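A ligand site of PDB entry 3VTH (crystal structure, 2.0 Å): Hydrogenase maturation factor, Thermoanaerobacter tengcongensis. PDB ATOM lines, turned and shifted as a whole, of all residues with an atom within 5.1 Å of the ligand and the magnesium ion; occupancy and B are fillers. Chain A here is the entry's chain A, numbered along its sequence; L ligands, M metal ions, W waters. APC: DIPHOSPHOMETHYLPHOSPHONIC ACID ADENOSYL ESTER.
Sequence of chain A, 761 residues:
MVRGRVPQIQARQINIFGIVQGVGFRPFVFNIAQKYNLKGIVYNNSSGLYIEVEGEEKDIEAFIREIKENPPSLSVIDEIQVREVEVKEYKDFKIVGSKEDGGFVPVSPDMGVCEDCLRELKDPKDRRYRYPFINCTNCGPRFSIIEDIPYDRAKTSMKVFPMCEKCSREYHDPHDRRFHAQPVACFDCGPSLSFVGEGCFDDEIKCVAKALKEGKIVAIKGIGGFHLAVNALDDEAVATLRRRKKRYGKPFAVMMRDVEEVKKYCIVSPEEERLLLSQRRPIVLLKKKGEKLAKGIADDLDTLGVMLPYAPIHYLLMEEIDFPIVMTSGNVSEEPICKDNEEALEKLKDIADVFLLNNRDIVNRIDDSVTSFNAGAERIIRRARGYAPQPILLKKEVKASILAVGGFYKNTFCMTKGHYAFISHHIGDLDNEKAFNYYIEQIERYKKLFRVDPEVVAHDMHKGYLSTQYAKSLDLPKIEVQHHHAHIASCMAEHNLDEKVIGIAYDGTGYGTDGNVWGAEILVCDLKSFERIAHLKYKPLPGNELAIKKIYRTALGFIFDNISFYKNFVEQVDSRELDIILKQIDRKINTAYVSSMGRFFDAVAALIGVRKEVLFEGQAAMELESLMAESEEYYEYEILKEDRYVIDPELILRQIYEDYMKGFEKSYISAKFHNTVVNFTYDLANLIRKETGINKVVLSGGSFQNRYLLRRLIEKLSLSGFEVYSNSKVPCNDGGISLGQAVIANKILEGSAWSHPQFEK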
ATOM      1  N   LYS A 245     -14.047 -14.485 -15.351  1.00  0.00           N
ATOM      2  CA  LYS A 245     -14.749 -13.769 -16.420  1.00  0.00           C
ATOM      3  C   LYS A 245     -14.546 -12.245 -16.309  1.00  0.00           C
ATOM      4  O   LYS A 245     -14.644 -11.525 -17.316  1.00  0.00           O
ATOM      5  CB  LYS A 245     -16.237 -14.143 -16.484  1.00  0.00           C
ATOM      6  CG  LYS A 245     -16.929 -13.701 -17.787  1.00  0.00           C
ATOM      7  CD  LYS A 245     -18.374 -14.187 -17.938  1.00  0.00           C
ATOM      8  CE  LYS A 245     -19.048 -13.476 -19.112  1.00  0.00           C
ATOM      9  NZ  LYS A 245     -20.435 -13.964 -19.371  1.00  0.00           N
ATOM     10  N   ARG A 247     -16.485 -10.351 -14.468  1.00  0.00           N
ATOM     11  CA  ARG A 247     -17.879  -9.867 -14.467  1.00  0.00           C
ATOM     12  C   ARG A 247     -18.325  -9.791 -13.018  1.00  0.00           C
ATOM     13  O   ARG A 247     -18.796 -10.782 -12.447  1.00  0.00           O
ATOM     14  CB  ARG A 247     -18.738 -10.869 -15.239  1.00  0.00           C
ATOM     15  CG  ARG A 247     -20.191 -10.480 -15.478  1.00  0.00           C
ATOM     16  CD  ARG A 247     -20.825 -11.625 -16.269  1.00  0.00           C
ATOM     17  NE  ARG A 247     -22.249 -11.446 -16.522  1.00  0.00           N
ATOM     18  CZ  ARG A 247     -23.203 -11.568 -15.608  1.00  0.00           C
ATOM     19  NH1 ARG A 247     -22.887 -11.840 -14.343  1.00  0.00           N
ATOM     20  NH2 ARG A 247     -24.471 -11.411 -15.941  1.00  0.00           N
ATOM     21  N   LYS A 250     -22.949  -7.558 -12.570  1.00  0.00           N
ATOM     22  CA  LYS A 250     -24.152  -7.979 -13.273  1.00  0.00           C
ATOM     23  C   LYS A 250     -24.629  -9.330 -12.710  1.00  0.00           C
ATOM     24  O   LYS A 250     -23.819 -10.240 -12.535  1.00  0.00           O
ATOM     25  CB  LYS A 250     -23.897  -8.128 -14.778  1.00  0.00           C
ATOM     26  CG  LYS A 250     -23.849  -6.831 -15.591  1.00  0.00           C
ATOM     27  CD  LYS A 250     -23.894  -7.206 -17.087  1.00  0.00           C
ATOM     28  CE  LYS A 250     -23.802  -5.976 -18.010  1.00  0.00           C
ATOM     29  NZ  LYS A 250     -23.632  -6.397 -19.438  1.00  0.00           N
ATOM     30  N   PRO A 251     -25.941  -9.448 -12.436  1.00  0.00           N
ATOM     31  CA  PRO A 251     -26.490 -10.712 -11.903  1.00  0.00           C
ATOM     32  C   PRO A 251     -26.356 -11.870 -12.883  1.00  0.00           C
ATOM     33  O   PRO A 251     -26.428 -11.657 -14.100  1.00  0.00           O
ATOM     34  CB  PRO A 251     -27.986 -10.393 -11.699  1.00  0.00           C
ATOM     35  CG  PRO A 251     -28.259  -9.260 -12.719  1.00  0.00           C
ATOM     36  CD  PRO A 251     -26.995  -8.456 -12.729  1.00  0.00           C
ATOM     37  N   PHE A 252     -26.174 -13.068 -12.349  1.00  0.00           N
ATOM     38  CA  PHE A 252     -26.164 -14.285 -13.144  1.00  0.00           C
ATOM     39  C   PHE A 252     -27.548 -14.900 -13.220  1.00  0.00           C
ATOM     40  O   PHE A 252     -28.243 -15.037 -12.189  1.00  0.00           O
ATOM     41  CB  PHE A 252     -25.264 -15.347 -12.503  1.00  0.00           C
ATOM     42  CG  PHE A 252     -23.791 -15.103 -12.671  1.00  0.00           C
ATOM     43  CD1 PHE A 252     -23.253 -14.729 -13.904  1.00  0.00           C
ATOM     44  CD2 PHE A 252     -22.927 -15.305 -11.600  1.00  0.00           C
ATOM     45  CE1 PHE A 252     -21.872 -14.543 -14.047  1.00  0.00           C
ATOM     46  CE2 PHE A 252     -21.556 -15.120 -11.742  1.00  0.00           C
ATOM     47  CZ  PHE A 252     -21.029 -14.719 -12.950  1.00  0.00           C
ATOM     48  N   ALA A 253     -27.920 -15.310 -14.427  1.00  0.00           N
ATOM     49  CA  ALA A 253     -29.075 -16.156 -14.654  1.00  0.00           C
ATOM     50  C   ALA A 253     -28.742 -17.588 -14.242  1.00  0.00           C
ATOM     51  O   ALA A 253     -27.596 -18.000 -14.315  1.00  0.00           O
ATOM     52  CB  ALA A 253     -29.463 -16.119 -16.126  1.00  0.00           C
ATOM     53  N   ILE A 283     -34.715 -16.994 -20.286  1.00  0.00           N
ATOM     54  CA  ILE A 283     -34.520 -16.604 -18.880  1.00  0.00           C
ATOM     55  C   ILE A 283     -35.732 -15.712 -18.524  1.00  0.00           C
ATOM     56  O   ILE A 283     -36.081 -14.831 -19.285  1.00  0.00           O
ATOM     57  CB  ILE A 283     -33.225 -15.759 -18.759  1.00  0.00           C
ATOM     58  CG1 ILE A 283     -31.992 -16.628 -19.082  1.00  0.00           C
ATOM     59  CG2 ILE A 283     -33.131 -15.082 -17.366  1.00  0.00           C
ATOM     60  CD1 ILE A 283     -30.767 -15.823 -19.519  1.00  0.00           C
ATOM     61  N   LEU A 285     -37.336 -13.200 -15.534  1.00  0.00           N
ATOM     62  CA  LEU A 285     -37.051 -12.488 -14.293  1.00  0.00           C
ATOM     63  C   LEU A 285     -38.205 -12.660 -13.316  1.00  0.00           C
ATOM     64  O   LEU A 285     -39.348 -12.300 -13.615  1.00  0.00           O
ATOM     65  CB  LEU A 285     -36.775 -10.993 -14.545  1.00  0.00           C
ATOM     66  CG  LEU A 285     -35.669 -10.705 -15.573  1.00  0.00           C
ATOM     67  CD1 LEU A 285     -35.457  -9.220 -15.681  1.00  0.00           C
ATOM     68  CD2 LEU A 285     -34.342 -11.423 -15.216  1.00  0.00           C
ATOM     69  N   ALA A 298     -27.240 -12.791  -7.360  1.00  0.00           N
ATOM     70  CA  ALA A 298     -28.018 -11.584  -7.615  1.00  0.00           C
ATOM     71  C   ALA A 298     -28.136 -10.762  -6.350  1.00  0.00           C
ATOM     72  O   ALA A 298     -29.233 -10.407  -5.909  1.00  0.00           O
ATOM     73  CB  ALA A 298     -29.403 -11.949  -8.182  1.00  0.00           C
ATOM     74  N   LEU A 301     -30.499  -7.435  -5.352  1.00  0.00           N
ATOM     75  CA  LEU A 301     -31.682  -7.396  -6.181  1.00  0.00           C
ATOM     76  C   LEU A 301     -32.778  -8.258  -5.562  1.00  0.00           C
ATOM     77  O   LEU A 301     -32.484  -9.213  -4.816  1.00  0.00           O
ATOM     78  CB  LEU A 301     -31.366  -7.860  -7.610  1.00  0.00           C
ATOM     79  CG  LEU A 301     -30.266  -7.072  -8.344  1.00  0.00           C
ATOM     80  CD1 LEU A 301     -29.980  -7.682  -9.717  1.00  0.00           C
ATOM     81  CD2 LEU A 301     -30.631  -5.606  -8.470  1.00  0.00           C
ATOM     82  N   THR A 303     -34.987  -9.836  -7.480  1.00  0.00           N
ATOM     83  CA  THR A 303     -35.356 -10.744  -8.562  1.00  0.00           C
ATOM     84  C   THR A 303     -34.229 -11.713  -8.930  1.00  0.00           C
ATOM     85  O   THR A 303     -33.062 -11.443  -8.671  1.00  0.00           O
ATOM     86  CB  THR A 303     -35.724  -9.983  -9.851  1.00  0.00           C
ATOM     87  OG1 THR A 303     -34.584  -9.200 -10.252  1.00  0.00           O
ATOM     88  CG2 THR A 303     -36.958  -9.041  -9.643  1.00  0.00           C
ATOM     89  N   LEU A 304     -34.607 -12.850  -9.516  1.00  0.00           N
ATOM     90  CA  LEU A 304     -33.659 -13.823 -10.035  1.00  0.00           C
ATOM     91  C   LEU A 304     -34.028 -14.065 -11.500  1.00  0.00           C
ATOM     92  O   LEU A 304     -35.217 -14.110 -11.844  1.00  0.00           O
ATOM     93  CB  LEU A 304     -33.821 -15.120  -9.244  1.00  0.00           C
ATOM     94  CG  LEU A 304     -32.670 -15.960  -8.679  1.00  0.00           C
ATOM     95  CD1 LEU A 304     -31.494 -15.134  -8.124  1.00  0.00           C
ATOM     96  CD2 LEU A 304     -33.257 -16.889  -7.572  1.00  0.00           C
ATOM     97  N   GLY A 305     -33.017 -14.245 -12.361  1.00  0.00           N
ATOM     98  CA  GLY A 305     -33.252 -14.624 -13.746  1.00  0.00           C
ATOM     99  C   GLY A 305     -33.160 -16.132 -13.825  1.00  0.00           C
ATOM    100  O   GLY A 305     -32.117 -16.705 -13.528  1.00  0.00           O
ATOM    101  N   MET A 327     -25.756 -20.065 -15.679  1.00  0.00           N
ATOM    102  CA  MET A 327     -25.479 -20.134 -17.095  1.00  0.00           C
ATOM    103  C   MET A 327     -25.197 -18.709 -17.526  1.00  0.00           C
ATOM    104  O   MET A 327     -26.114 -17.876 -17.555  1.00  0.00           O
ATOM    105  CB  MET A 327     -26.677 -20.690 -17.873  1.00  0.00           C
ATOM    106  CG  MET A 327     -26.909 -22.172 -17.670  1.00  0.00           C
ATOM    107  SD  MET A 327     -25.601 -23.123 -18.467  1.00  0.00           S
ATOM    108  CE  MET A 327     -26.376 -23.483 -20.051  1.00  0.00           C
ATOM    109  N   THR A 328     -23.947 -18.420 -17.835  1.00  0.00           N
ATOM    110  CA  THR A 328     -23.546 -17.103 -18.297  1.00  0.00           C
ATOM    111  C   THR A 328     -22.858 -17.321 -19.621  1.00  0.00           C
ATOM    112  O   THR A 328     -22.323 -18.397 -19.864  1.00  0.00           O
ATOM    113  CB  THR A 328     -22.661 -16.347 -17.257  1.00  0.00           C
ATOM    114  OG1 THR A 328     -22.473 -14.986 -17.682  1.00  0.00           O
ATOM    115  CG2 THR A 328     -21.299 -17.018 -17.084  1.00  0.00           C
ATOM    116  N   SER A 329     -22.878 -16.324 -20.496  1.00  0.00           N
ATOM    117  CA  SER A 329     -22.383 -16.563 -21.839  1.00  0.00           C
ATOM    118  C   SER A 329     -20.860 -16.779 -21.804  1.00  0.00           C
ATOM    119  O   SER A 329     -20.148 -16.184 -20.994  1.00  0.00           O
ATOM    120  CB  SER A 329     -22.792 -15.420 -22.797  1.00  0.00           C
ATOM    121  OG  SER A 329     -22.143 -14.218 -22.442  1.00  0.00           O
ATOM    122  N   ASN A 331     -17.661 -16.104 -22.855  1.00  0.00           N
ATOM    123  CA  ASN A 331     -16.790 -15.086 -23.448  1.00  0.00           C
ATOM    124  C   ASN A 331     -16.093 -14.359 -22.310  1.00  0.00           C
ATOM    125  O   ASN A 331     -16.528 -14.437 -21.151  1.00  0.00           O
ATOM    126  CB  ASN A 331     -17.595 -14.104 -24.303  1.00  0.00           C
ATOM    127  CG  ASN A 331     -18.878 -13.632 -23.619  1.00  0.00           C
ATOM    128  OD1 ASN A 331     -19.947 -14.210 -23.827  1.00  0.00           O
ATOM    129  ND2 ASN A 331     -18.781 -12.564 -22.811  1.00  0.00           N
ATOM    130  N   VAL A 332     -14.995 -13.658 -22.610  1.00  0.00           N
ATOM    131  CA  VAL A 332     -14.483 -12.699 -21.639  1.00  0.00           C
ATOM    132  C   VAL A 332     -15.506 -11.566 -21.631  1.00  0.00           C
ATOM    133  O   VAL A 332     -16.168 -11.291 -22.648  1.00  0.00           O
ATOM    134  CB  VAL A 332     -13.012 -12.232 -21.904  1.00  0.00           C
ATOM    135  CG1 VAL A 332     -12.778 -11.797 -23.338  1.00  0.00           C
ATOM    136  CG2 VAL A 332     -12.588 -11.106 -20.932  1.00  0.00           C
ATOM    137  N   SER A 333     -15.665 -10.944 -20.461  1.00  0.00           N
ATOM    138  CA  SER A 333     -16.571  -9.819 -20.315  1.00  0.00           C
ATOM    139  C   SER A 333     -16.483  -8.896 -21.544  1.00  0.00           C
ATOM    140  O   SER A 333     -15.384  -8.573 -21.996  1.00  0.00           O
ATOM    141  CB  SER A 333     -16.257  -9.039 -19.033  1.00  0.00           C
ATOM    142  OG  SER A 333     -17.390  -8.282 -18.634  1.00  0.00           O
ATOM    143  N   GLU A 334     -17.646  -8.538 -22.102  1.00  0.00           N
ATOM    144  CA  GLU A 334     -17.820  -7.515 -23.150  1.00  0.00           C
ATOM    145  C   GLU A 334     -17.532  -7.939 -24.609  1.00  0.00           C
ATOM    146  O   GLU A 334     -17.709  -7.155 -25.534  1.00  0.00           O
ATOM    147  CB  GLU A 334     -17.074  -6.201 -22.815  1.00  0.00           C
ATOM    148  CG  GLU A 334     -17.581  -5.524 -21.547  1.00  0.00           C
ATOM    149  CD  GLU A 334     -16.682  -4.389 -21.101  1.00  0.00           C
ATOM    150  OE1 GLU A 334     -16.715  -4.062 -19.886  1.00  0.00           O
ATOM    151  OE2 GLU A 334     -15.935  -3.832 -21.935  1.00  0.00           O
ATOM    152  N   GLU A 335     -17.125  -9.195 -24.799  1.00  0.00           N
ATOM    153  CA  GLU A 335     -16.928  -9.762 -26.124  1.00  0.00           C
ATOM    154  C   GLU A 335     -18.118 -10.658 -26.512  1.00  0.00           C
ATOM    155  O   GLU A 335     -18.769 -11.223 -25.641  1.00  0.00           O
ATOM    156  CB  GLU A 335     -15.612 -10.544 -26.177  1.00  0.00           C
ATOM    157  CG  GLU A 335     -14.370  -9.663 -26.052  1.00  0.00           C
ATOM    158  CD  GLU A 335     -13.045 -10.427 -26.194  1.00  0.00           C
ATOM    159  OE1 GLU A 335     -13.020 -11.573 -26.707  1.00  0.00           O
ATOM    160  OE2 GLU A 335     -12.021  -9.857 -25.770  1.00  0.00           O
ATOM    161  N   ASP A 367     -27.556 -15.266 -28.221  1.00  0.00           N
ATOM    162  CA  ASP A 367     -27.642 -15.338 -26.760  1.00  0.00           C
ATOM    163  C   ASP A 367     -28.990 -15.837 -26.256  1.00  0.00           C
ATOM    164  O   ASP A 367     -29.977 -15.829 -26.989  1.00  0.00           O
ATOM    165  CB  ASP A 367     -27.370 -13.944 -26.178  1.00  0.00           C
ATOM    166  CG  ASP A 367     -25.903 -13.615 -26.151  1.00  0.00           C
ATOM    167  OD1 ASP A 367     -25.152 -14.279 -25.404  1.00  0.00           O
ATOM    168  OD2 ASP A 367     -25.485 -12.715 -26.910  1.00  0.00           O
ATOM    169  N   VAL A 370     -33.996 -12.826 -22.416  1.00  0.00           N
ATOM    170  CA  VAL A 370     -34.358 -12.468 -21.047  1.00  0.00           C
ATOM    171  C   VAL A 370     -35.710 -11.789 -21.118  1.00  0.00           C
ATOM    172  O   VAL A 370     -35.883 -10.813 -21.849  1.00  0.00           O
ATOM    173  CB  VAL A 370     -33.314 -11.526 -20.388  1.00  0.00           C
ATOM    174  CG1 VAL A 370     -33.717 -11.185 -18.948  1.00  0.00           C
ATOM    175  CG2 VAL A 370     -31.897 -12.175 -20.426  1.00  0.00           C
ATOM    176  N   ARG A 382     -34.296  -8.803 -23.349  1.00  0.00           N
ATOM    177  CA  ARG A 382     -33.273  -9.140 -24.322  1.00  0.00           C
ATOM    178  C   ARG A 382     -33.913 -10.124 -25.285  1.00  0.00           C
ATOM    179  O   ARG A 382     -34.265 -11.228 -24.910  1.00  0.00           O
ATOM    180  CB  ARG A 382     -32.031  -9.723 -23.632  1.00  0.00           C
ATOM    181  CG  ARG A 382     -30.868 -10.055 -24.618  1.00  0.00           C
ATOM    182  CD  ARG A 382     -29.665 -10.661 -23.845  1.00  0.00           C
ATOM    183  NE  ARG A 382     -28.882  -9.626 -23.181  1.00  0.00           N
ATOM    184  CZ  ARG A 382     -27.717  -9.832 -22.563  1.00  0.00           C
ATOM    185  NH1 ARG A 382     -27.201 -11.064 -22.498  1.00  0.00           N
ATOM    186  NH2 ARG A 382     -27.057  -8.813 -22.009  1.00  0.00           N
ATOM    187  N   MET A 622     -31.522  -0.290 -10.409  1.00  0.00           N
ATOM    188  CA  MET A 622     -32.029  -1.616 -10.081  1.00  0.00           C
ATOM    189  C   MET A 622     -32.061  -1.867  -8.573  1.00  0.00           C
ATOM    190  O   MET A 622     -33.018  -2.415  -8.057  1.00  0.00           O
ATOM    191  CB  MET A 622     -31.194  -2.689 -10.791  1.00  0.00           C
ATOM    192  CG  MET A 622     -31.337  -2.636 -12.321  1.00  0.00           C
ATOM    193  SD  MET A 622     -30.147  -3.693 -13.181  1.00  0.00           S
ATOM    194  CE  MET A 622     -30.828  -5.304 -12.776  1.00  0.00           C
HETATM  195  PG  APC L   1     -21.000 -10.217 -20.639  1.00  0.00           P
HETATM  196  O1G APC L   1     -21.241 -11.616 -21.139  1.00  0.00           O
HETATM  197  O2G APC L   1     -20.502 -10.200 -19.213  1.00  0.00           O
HETATM  198  O3G APC L   1     -20.169  -9.367 -21.546  1.00  0.00           O
HETATM  199  PB  APC L   1     -23.869 -10.017 -20.428  1.00  0.00           P
HETATM  200  O1B APC L   1     -24.182 -10.703 -21.716  1.00  0.00           O
HETATM  201  O2B APC L   1     -24.766  -8.846 -20.086  1.00  0.00           O
HETATM  202  O3B APC L   1     -22.390  -9.402 -20.580  1.00  0.00           O
HETATM  203  PA  APC L   1     -24.682 -12.801 -19.218  1.00  0.00           P
HETATM  204  O1A APC L   1     -24.589 -13.504 -17.890  1.00  0.00           O
HETATM  205  O2A APC L   1     -24.224 -13.595 -20.395  1.00  0.00           O
HETATM  206  C3A APC L   1     -23.791 -11.211 -19.050  1.00  0.00           C
HETATM  207  O5' APC L   1     -26.208 -12.420 -19.562  1.00  0.00           O
HETATM  208  C5' APC L   1     -27.290 -12.567 -18.641  1.00  0.00           C
HETATM  209  C4' APC L   1     -28.164 -11.314 -18.723  1.00  0.00           C
HETATM  210  O4' APC L   1     -29.307 -11.558 -17.894  1.00  0.00           O
HETATM  211  C3' APC L   1     -27.433 -10.098 -18.171  1.00  0.00           C
HETATM  212  O3' APC L   1     -27.673  -8.916 -18.956  1.00  0.00           O
HETATM  213  C2' APC L   1     -28.062  -9.902 -16.803  1.00  0.00           C
HETATM  214  O2' APC L   1     -27.942  -8.539 -16.335  1.00  0.00           O
HETATM  215  C1' APC L   1     -29.470 -10.432 -17.017  1.00  0.00           C
HETATM  216  N9  APC L   1     -29.965 -10.841 -15.704  1.00  0.00           N
HETATM  217  C8  APC L   1     -29.619 -11.958 -14.999  1.00  0.00           C
HETATM  218  N7  APC L   1     -30.249 -11.945 -13.798  1.00  0.00           N
HETATM  219  C5  APC L   1     -30.992 -10.823 -13.738  1.00  0.00           C
HETATM  220  C6  APC L   1     -31.895 -10.176 -12.762  1.00  0.00           C
HETATM  221  N6  APC L   1     -32.154 -10.757 -11.576  1.00  0.00           N
HETATM  222  N1  APC L   1     -32.458  -8.995 -13.101  1.00  0.00           N
HETATM  223  C2  APC L   1     -32.241  -8.400 -14.287  1.00  0.00           C
HETATM  224  N3  APC L   1     -31.429  -8.913 -15.232  1.00  0.00           N
HETATM  225  C4  APC L   1     -30.798 -10.095 -15.003  1.00  0.00           C
HETATM  226 MG    MG M   1     -23.074 -12.389 -21.904  1.00  0.00          MG
HETATM  227  O   HOH W   1     -34.476  -7.461 -12.162  1.00  0.00           O
HETATM  228  O   HOH W   2     -26.934  -6.209 -19.217  1.00  0.00           O
HETATM  229  O   HOH W   3     -26.733 -15.168 -21.410  1.00  0.00           O
HETATM  230  O   HOH W   4     -30.368 -13.510 -11.562  1.00  0.00           O
HETATM  231  O   HOH W   5     -20.092  -7.917 -17.805  1.00  0.00           O
HETATM  232  O   HOH W   6     -25.905 -15.253 -16.448  1.00  0.00           O
HETATM  233  O   HOH W   7     -22.417 -11.831 -23.954  1.00  0.00           O
HETATM  234  O   HOH W   8     -30.432  -8.154 -20.006  1.00  0.00           O
HETATM  235  O   HOH W   9     -24.269  -9.369 -24.263  1.00  0.00           O
HETATM  236  O   HOH W  10     -20.463  -9.932 -23.864  1.00  0.00           O
HETATM  237  O   HOH W  11     -31.375  -7.321 -17.564  1.00  0.00           O
HETATM  238  O   HOH W  12     -28.743  -6.075 -17.175  1.00  0.00           O
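The backbone NH (N) of Ser 329 lies close to an oxygen (O2A) of the ligand, 3.0 Å away. An oxygen (O1A) of the ligand is in hydrogen-bond range of the side-chain hydroxyl (OG1) of Thr 328. The backbone NH (N) of Glu 334 lies within hydrogen-bond range of an oxygen (O3G) of the ligand (2.7 Å). The side-chain amino group (NZ) of Lys 250 lies within salt-bridge range of an oxygen (O2B) of the ligand (2.8 Å). An oxygen (O1A) of the ligand lies within salt-bridge range of the guanidinium group (NH2) of Arg 247, 2.9 Å away. The guanidinium group of Arg 382 lies within salt-bridge range of an oxygen (O2B) of the ligand. The side-chain amino group (NZ) of Lys 245 lies within salt-bridge range of an oxygen (O2G) of the ligand, 3.8 Å away. The backbone carbonyl oxygen of Thr 303 sits at hydrogen-bond distance from a nitrogen (N6) of the ligand (3.1 Å). The side-chain hydroxyl of Thr 303 sits at hydrogen-bond distance from a nitrogen (N6) of the ligand (3.2 Å). The side-chain amide nitrogen of Asn 331 sits close to an oxygen (O1G) of the ligand, at 3.1 Å.
O of Ser 329 lies within hydrogen-bond range of NZ of Lys 245, 2.8 Å away. O of Ser 329 lies close to OD1 of Asn 331 (3.5 Å). NZ of Lys 245 lies within hydrogen-bond range of OG1 of Thr 328 (2.8 Å). The backbone carbonyl oxygen (O) of Lys 250 is in hydrogen-bond range of the guanidinium group (NH1) of Arg 247 (2.6 Å). N of Arg 382 sits at hydrogen-bond distance from O of Val 370 (3.0 Å). O of Lys 245 sits at hydrogen-bond distance from N of Ser 333. The side-chain amide nitrogen of Asn 331 sits at hydrogen-bond distance from the backbone carbonyl oxygen of Glu 335, at 3.1 Å. The backbone carbonyl oxygen of Ala 253 is in hydrogen-bond range of the backbone NH of Met 327, at 3.1 Å.
Merely in contact with the ligand: Pro 251 (3.3 Å), Ala 253 (3.8 Å), Leu 285 (3.6 Å), Leu 304 (3.7 Å), Gly 305 (3.7 Å), Ser 333 (3.7 Å), Val 370 (3.7 Å) and Met 622 (3.7 Å). Hydrophobic or aromatic side chains that line the ligand: Pro 251, Leu 285, Val 370 and Met 622. Of the 25 residues printed, 17 come within 4 Å of the ligand. The nearest printed residue that does not touch the ligand is Phe 252 (4.01 Å).
Lys 245 touches the magnesium ion.
The magnesium ion is bound by O1B of the ligand (2.0 Å). OG of Ser 329 is bound to the magnesium ion (2.1 Å). O1G of the ligand binds the magnesium ion, at 2.1 Å. Water W7 is bound to the magnesium ion (2.2 Å). O2A of the ligand binds the magnesium ion, at 2.2 Å. The magnesium ion has five donor atoms within binding distance.
Water W10 lies within hydrogen-bond range of O3G of the ligand (2.4 Å), O of Glu 335 (2.8 Å) and ND2 of Asn 331 (3.3 Å). Water W6 lies within hydrogen-bond range of O1A of the ligand (2.6 Å), O of Met 327 (2.9 Å) and N of Ala 253 (2.9 Å). Water W1 lies within hydrogen-bond range of OG1 of Thr 303 (2.6 Å) and N1 of the ligand (2.7 Å). Water W5 lies within hydrogen-bond range of an oxygen (O2G) of the ligand and the side-chain hydroxyl (OG) of Ser 333. Water W4 lies within hydrogen-bond range of the backbone carbonyl oxygen of Phe 252 (2.7 Å), a nitrogen (N7) of the ligand (2.7 Å) and the backbone NH of Gly 305 (2.9 Å). Water W2 lies within hydrogen-bond range of O3' of the ligand (2.8 Å) and NZ of Lys 250 (3.3 Å).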
